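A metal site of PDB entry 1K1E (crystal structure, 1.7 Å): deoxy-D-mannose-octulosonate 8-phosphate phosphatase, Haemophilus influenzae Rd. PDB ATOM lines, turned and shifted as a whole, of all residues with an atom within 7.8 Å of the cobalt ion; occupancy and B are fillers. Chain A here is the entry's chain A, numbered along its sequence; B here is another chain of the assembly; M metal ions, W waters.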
ATOM      1  N   ASP A  14      -4.752 -24.920 -13.261  1.00  0.00           N
ATOM      2  CA  ASP A  14      -3.886 -25.681 -12.387  1.00  0.00           C
ATOM      3  C   ASP A  14      -4.003 -24.950 -11.042  1.00  0.00           C
ATOM      4  O   ASP A  14      -4.507 -23.821 -10.948  1.00  0.00           O
ATOM      5  CB  ASP A  14      -2.411 -25.576 -12.883  1.00  0.00           C
ATOM      6  CG  ASP A  14      -1.426 -26.052 -11.858  1.00  0.00           C
ATOM      7  OD1 ASP A  14      -1.695 -27.067 -11.195  1.00  0.00           O
ATOM      8  OD2 ASP A  14      -0.368 -25.421 -11.733  1.00  0.00           O
ATOM      9  N   VAL A  15      -3.590 -25.604  -9.960  1.00  0.00           N
ATOM     10  CA  VAL A  15      -3.652 -24.952  -8.667  1.00  0.00           C
ATOM     11  C   VAL A  15      -2.334 -24.381  -8.129  1.00  0.00           C
ATOM     12  O   VAL A  15      -2.176 -23.168  -8.005  1.00  0.00           O
ATOM     13  CB  VAL A  15      -4.222 -25.943  -7.553  1.00  0.00           C
ATOM     14  CG1 VAL A  15      -4.132 -25.310  -6.162  1.00  0.00           C
ATOM     15  CG2 VAL A  15      -5.685 -26.258  -7.900  1.00  0.00           C
ATOM     16  N   ASP A  16      -1.391 -25.246  -7.813  1.00  0.00           N
ATOM     17  CA  ASP A  16      -0.161 -24.725  -7.183  1.00  0.00           C
ATOM     18  C   ASP A  16       0.688 -23.973  -8.144  1.00  0.00           C
ATOM     19  O   ASP A  16       1.058 -24.514  -9.154  1.00  0.00           O
ATOM     20  CB  ASP A  16       0.625 -25.870  -6.560  1.00  0.00           C
ATOM     21  CG  ASP A  16      -0.191 -26.574  -5.479  1.00  0.00           C
ATOM     22  OD1 ASP A  16      -0.545 -25.878  -4.495  1.00  0.00           O
ATOM     23  OD2 ASP A  16      -0.536 -27.765  -5.660  1.00  0.00           O
ATOM     24  N   GLY A  17       0.999 -22.725  -7.835  1.00  0.00           N
ATOM     25  CA  GLY A  17       1.857 -21.972  -8.756  1.00  0.00           C
ATOM     26  C   GLY A  17       1.047 -21.093  -9.678  1.00  0.00           C
ATOM     27  O   GLY A  17       1.619 -20.202 -10.344  1.00  0.00           O
ATOM     28  N   VAL A  18      -0.285 -21.337  -9.709  1.00  0.00           N
ATOM     29  CA  VAL A  18      -1.180 -20.546 -10.527  1.00  0.00           C
ATOM     30  C   VAL A  18      -2.170 -19.866  -9.599  1.00  0.00           C
ATOM     31  O   VAL A  18      -2.150 -18.650  -9.499  1.00  0.00           O
ATOM     32  CB  VAL A  18      -1.891 -21.413 -11.568  1.00  0.00           C
ATOM     33  CG1 VAL A  18      -2.934 -20.615 -12.317  1.00  0.00           C
ATOM     34  CG2 VAL A  18      -0.838 -21.889 -12.598  1.00  0.00           C
ATOM     35  N   LEU A  19      -2.974 -20.633  -8.877  1.00  0.00           N
ATOM     36  CA  LEU A  19      -3.912 -20.005  -7.929  1.00  0.00           C
ATOM     37  C   LEU A  19      -3.188 -19.688  -6.605  1.00  0.00           C
ATOM     38  O   LEU A  19      -3.752 -19.008  -5.751  1.00  0.00           O
ATOM     39  CB  LEU A  19      -5.076 -20.938  -7.631  1.00  0.00           C
ATOM     40  CG  LEU A  19      -5.938 -21.222  -8.884  1.00  0.00           C
ATOM     41  CD1 LEU A  19      -7.128 -22.130  -8.357  1.00  0.00           C
ATOM     42  CD2 LEU A  19      -6.504 -19.870  -9.437  1.00  0.00           C
ATOM     43  N   THR A  20      -1.981 -20.195  -6.453  1.00  0.00           N
ATOM     44  CA  THR A  20      -1.107 -19.968  -5.298  1.00  0.00           C
ATOM     45  C   THR A  20       0.265 -19.480  -5.828  1.00  0.00           C
ATOM     46  O   THR A  20       0.519 -19.543  -7.047  1.00  0.00           O
ATOM     47  CB  THR A  20      -0.843 -21.245  -4.484  1.00  0.00           C
ATOM     48  OG1 THR A  20       0.127 -22.033  -5.165  1.00  0.00           O
ATOM     49  CG2 THR A  20      -2.143 -22.046  -4.226  1.00  0.00           C
ATOM     50  N   GLY A  22       2.854 -20.961  -5.341  1.00  0.00           N
ATOM     51  CA  GLY A  22       3.718 -22.139  -5.415  1.00  0.00           C
ATOM     52  C   GLY A  22       4.205 -22.710  -4.097  1.00  0.00           C
ATOM     53  O   GLY A  22       4.787 -23.787  -4.062  1.00  0.00           O
ATOM     54  N   LEU A  57      -7.741 -28.347 -11.789  1.00  0.00           N
ATOM     55  CA  LEU A  57      -7.043 -29.581 -12.095  1.00  0.00           C
ATOM     56  C   LEU A  57      -5.810 -29.536 -11.196  1.00  0.00           C
ATOM     57  O   LEU A  57      -5.068 -28.581 -11.249  1.00  0.00           O
ATOM     58  CB  LEU A  57      -6.628 -29.553 -13.563  1.00  0.00           C
ATOM     59  CG  LEU A  57      -6.628 -30.821 -14.408  1.00  0.00           C
ATOM     60  CD1 LEU A  57      -5.650 -30.603 -15.512  1.00  0.00           C
ATOM     61  CD2 LEU A  57      -6.237 -32.076 -13.636  1.00  0.00           C
ATOM     62  N   SER A  58      -5.613 -30.517 -10.333  1.00  0.00           N
ATOM     63  CA  SER A  58      -4.425 -30.496  -9.494  1.00  0.00           C
ATOM     64  C   SER A  58      -3.955 -31.929  -9.304  1.00  0.00           C
ATOM     65  O   SER A  58      -4.784 -32.836  -9.239  1.00  0.00           O
ATOM     66  CB  SER A  58      -4.759 -29.920  -8.100  1.00  0.00           C
ATOM     67  OG  SER A  58      -3.635 -30.003  -7.268  1.00  0.00           O
ATOM     68  N   GLY A  59      -2.639 -32.128  -9.260  1.00  0.00           N
ATOM     69  CA  GLY A  59      -2.105 -33.458  -9.033  1.00  0.00           C
ATOM     70  C   GLY A  59      -2.220 -33.847  -7.547  1.00  0.00           C
ATOM     71  O   GLY A  59      -1.843 -34.956  -7.139  1.00  0.00           O
ATOM     72  N   LYS A  84      -2.182 -34.849 -16.570  1.00  0.00           N
ATOM     73  CA  LYS A  84      -3.154 -33.834 -16.919  1.00  0.00           C
ATOM     74  C   LYS A  84      -3.778 -33.821 -18.303  1.00  0.00           C
ATOM     75  O   LYS A  84      -4.873 -33.305 -18.440  1.00  0.00           O
ATOM     76  CB  LYS A  84      -2.564 -32.444 -16.592  1.00  0.00           C
ATOM     77  CG  LYS A  84      -2.288 -32.323 -15.101  1.00  0.00           C
ATOM     78  CD  LYS A  84      -1.853 -30.900 -14.717  1.00  0.00           C
ATOM     79  CE  LYS A  84      -1.548 -30.816 -13.191  1.00  0.00           C
ATOM     80  NZ  LYS A  84      -1.443 -29.363 -12.837  1.00  0.00           N
ATOM     81  N   TYR A 104      -6.410 -23.011 -20.708  1.00  0.00           N
ATOM     82  CA  TYR A 104      -5.749 -23.607 -19.554  1.00  0.00           C
ATOM     83  C   TYR A 104      -4.721 -22.613 -19.027  1.00  0.00           C
ATOM     84  O   TYR A 104      -4.142 -21.884 -19.801  1.00  0.00           O
ATOM     85  CB  TYR A 104      -4.948 -24.836 -19.953  1.00  0.00           C
ATOM     86  CG  TYR A 104      -4.418 -25.647 -18.808  1.00  0.00           C
ATOM     87  CD1 TYR A 104      -5.192 -26.654 -18.188  1.00  0.00           C
ATOM     88  CD2 TYR A 104      -3.142 -25.388 -18.258  1.00  0.00           C
ATOM     89  CE1 TYR A 104      -4.720 -27.372 -17.060  1.00  0.00           C
ATOM     90  CE2 TYR A 104      -2.687 -26.095 -17.197  1.00  0.00           C
ATOM     91  CZ  TYR A 104      -3.441 -27.063 -16.588  1.00  0.00           C
ATOM     92  OH  TYR A 104      -2.936 -27.745 -15.511  1.00  0.00           O
ATOM     93  N   ILE A 105      -4.469 -22.636 -17.730  1.00  0.00           N
ATOM     94  CA  ILE A 105      -3.455 -21.744 -17.186  1.00  0.00           C
ATOM     95  C   ILE A 105      -2.580 -22.587 -16.275  1.00  0.00           C
ATOM     96  O   ILE A 105      -3.097 -23.229 -15.350  1.00  0.00           O
ATOM     97  CB  ILE A 105      -4.072 -20.488 -16.443  1.00  0.00           C
ATOM     98  CG1 ILE A 105      -2.913 -19.643 -15.818  1.00  0.00           C
ATOM     99  CG2 ILE A 105      -5.268 -20.884 -15.508  1.00  0.00           C
ATOM    100  CD1 ILE A 105      -3.448 -18.262 -15.257  1.00  0.00           C
ATOM    101  N   GLY A 106      -1.262 -22.571 -16.497  1.00  0.00           N
ATOM    102  CA  GLY A 106      -0.406 -23.444 -15.694  1.00  0.00           C
ATOM    103  C   GLY A 106       0.905 -22.752 -15.443  1.00  0.00           C
ATOM    104  O   GLY A 106       1.108 -21.598 -15.890  1.00  0.00           O
ATOM    105  N   ASP A 107       1.748 -23.434 -14.701  1.00  0.00           N
ATOM    106  CA  ASP A 107       3.067 -22.835 -14.359  1.00  0.00           C
ATOM    107  C   ASP A 107       4.265 -23.765 -14.506  1.00  0.00           C
ATOM    108  O   ASP A 107       5.392 -23.306 -14.356  1.00  0.00           O
ATOM    109  CB  ASP A 107       3.117 -22.381 -12.904  1.00  0.00           C
ATOM    110  CG  ASP A 107       3.098 -23.561 -11.922  1.00  0.00           C
ATOM    111  OD1 ASP A 107       3.927 -23.643 -10.996  1.00  0.00           O
ATOM    112  OD2 ASP A 107       2.222 -24.421 -12.055  1.00  0.00           O
ATOM    113  N   ASP A 108       4.028 -25.056 -14.720  1.00  0.00           N
ATOM    114  CA  ASP A 108       5.181 -25.985 -14.741  1.00  0.00           C
ATOM    115  C   ASP A 108       5.113 -27.101 -15.760  1.00  0.00           C
ATOM    116  O   ASP A 108       4.127 -27.205 -16.527  1.00  0.00           O
ATOM    117  CB  ASP A 108       5.375 -26.580 -13.304  1.00  0.00           C
ATOM    118  CG  ASP A 108       6.835 -26.945 -12.993  1.00  0.00           C
ATOM    119  OD1 ASP A 108       7.067 -27.420 -11.841  1.00  0.00           O
ATOM    120  OD2 ASP A 108       7.717 -26.736 -13.874  1.00  0.00           O
ATOM    121  N   SER A 109       6.163 -27.930 -15.762  1.00  0.00           N
ATOM    122  CA  SER A 109       6.282 -29.039 -16.726  1.00  0.00           C
ATOM    123  C   SER A 109       5.069 -29.920 -16.769  1.00  0.00           C
ATOM    124  O   SER A 109       4.665 -30.347 -17.874  1.00  0.00           O
ATOM    125  CB  SER A 109       7.536 -29.879 -16.419  1.00  0.00           C
ATOM    126  OG  SER A 109       8.687 -29.000 -16.427  1.00  0.00           O
ATOM    127  N   VAL A 110       4.491 -30.191 -15.603  1.00  0.00           N
ATOM    128  CA  VAL A 110       3.297 -31.044 -15.507  1.00  0.00           C
ATOM    129  C   VAL A 110       2.190 -30.479 -16.376  1.00  0.00           C
ATOM    130  O   VAL A 110       1.356 -31.228 -16.815  1.00  0.00           O
ATOM    131  CB  VAL A 110       2.726 -31.128 -14.021  1.00  0.00           C
ATOM    132  CG1 VAL A 110       1.795 -32.377 -13.843  1.00  0.00           C
ATOM    133  CG2 VAL A 110       3.883 -31.184 -12.993  1.00  0.00           C
ATOM    134  N   ASP A 111       2.153 -29.165 -16.607  1.00  0.00           N
ATOM    135  CA  ASP A 111       1.058 -28.618 -17.404  1.00  0.00           C
ATOM    136  C   ASP A 111       1.302 -28.626 -18.913  1.00  0.00           C
ATOM    137  O   ASP A 111       0.389 -28.310 -19.687  1.00  0.00           O
ATOM    138  CB  ASP A 111       0.804 -27.177 -16.953  1.00  0.00           C
ATOM    139  CG  ASP A 111       0.608 -27.085 -15.485  1.00  0.00           C
ATOM    140  OD1 ASP A 111      -0.320 -27.757 -15.004  1.00  0.00           O
ATOM    141  OD2 ASP A 111       1.363 -26.379 -14.779  1.00  0.00           O
ATOM    142  N   VAL A 124       1.708 -18.296 -16.127  1.00  0.00           N
ATOM    143  CA  VAL A 124       1.935 -17.239 -15.140  1.00  0.00           C
ATOM    144  C   VAL A 124       3.324 -16.657 -15.357  1.00  0.00           C
ATOM    145  O   VAL A 124       4.210 -17.314 -15.939  1.00  0.00           O
ATOM    146  CB  VAL A 124       1.797 -17.754 -13.670  1.00  0.00           C
ATOM    147  CG1 VAL A 124       0.356 -18.210 -13.449  1.00  0.00           C
ATOM    148  CG2 VAL A 124       2.762 -18.936 -13.396  1.00  0.00           C
ATOM    149  N   VAL B  38       6.644 -25.819  -4.671  1.00  0.00           N
ATOM    150  CA  VAL B  38       6.203 -26.944  -5.457  1.00  0.00           C
ATOM    151  C   VAL B  38       7.126 -27.245  -6.653  1.00  0.00           C
ATOM    152  O   VAL B  38       7.356 -28.405  -6.971  1.00  0.00           O
ATOM    153  CB  VAL B  38       4.709 -26.759  -5.940  1.00  0.00           C
ATOM    154  CG1 VAL B  38       4.535 -25.581  -6.927  1.00  0.00           C
ATOM    155  CG2 VAL B  38       4.202 -28.026  -6.516  1.00  0.00           C
ATOM    156  N   ARG B  39       7.659 -26.221  -7.280  1.00  0.00           N
ATOM    157  CA  ARG B  39       8.506 -26.512  -8.412  1.00  0.00           C
ATOM    158  C   ARG B  39       9.856 -27.107  -7.998  1.00  0.00           C
ATOM    159  O   ARG B  39      10.485 -27.832  -8.798  1.00  0.00           O
ATOM    160  CB  ARG B  39       8.638 -25.296  -9.351  1.00  0.00           C
ATOM    161  CG  ARG B  39       7.256 -24.960 -10.097  1.00  0.00           C
ATOM    162  CD  ARG B  39       7.414 -23.891 -11.242  1.00  0.00           C
ATOM    163  NE  ARG B  39       7.910 -22.574 -10.770  1.00  0.00           N
ATOM    164  CZ  ARG B  39       7.134 -21.587 -10.305  1.00  0.00           C
ATOM    165  NH1 ARG B  39       5.805 -21.763 -10.234  1.00  0.00           N
ATOM    166  NH2 ARG B  39       7.664 -20.436  -9.924  1.00  0.00           N
HETATM  167 CO    CO M   1       1.426 -25.835 -10.828  1.00  0.00          CO
HETATM  168  O   HOH W   1       1.819 -27.390 -12.235  1.00  0.00           O
HETATM  169  O   HOH W   2       3.233 -25.961  -9.787  1.00  0.00           O
HETATM  170  O   HOH W   3       0.333 -27.286  -9.610  1.00  0.00           O
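The cobalt ion is bound by the side-chain carboxylate of Asp 107, the side-chain carboxylate of Asp 14, water W2, water W1, the backbone carbonyl oxygen of Asp 16 and water W3.
Asp 111 touches the cobalt ion.
Four residues have an atom within 4 Å of the cobalt ion: Asp 14, Asp 16, Asp 107 and Asp 111.
The nearest printed residue that does not touch the cobalt ion is Gly 17 (4.3 Å).
Water W3 lies within hydrogen-bond range of OD1 of Asp 14 and N of Asp 16.
The backbone NH (N) of Asp 107 is in hydrogen-bond range of the side-chain carboxylate (OD2) of Asp 111 (3.0 Å).
The guanidinium group (NH1) of Arg 39 of chain B lies within salt-bridge range of the side-chain carboxylate (OD1) of Asp 107 (2.8 Å).
The side-chain carboxylate (OD1) of Asp 14 lies within salt-bridge range of the side-chain amino group (NZ) of Lys 84, at 2.8 Å.
O of Ile 105 sits at hydrogen-bond distance from N of Asp 14 (3.2 Å).
OD2 of Asp 111 is in hydrogen-bond range of N of Asp 108 (3.0 Å).
The side-chain amino group (NZ) of Lys 84 lies within salt-bridge range of the side-chain carboxylate (OD1) of Asp 111.
The side-chain carboxylate (OD1) of Asp 111 sits at hydrogen-bond distance from the side-chain hydroxyl (OH) of Tyr 104.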
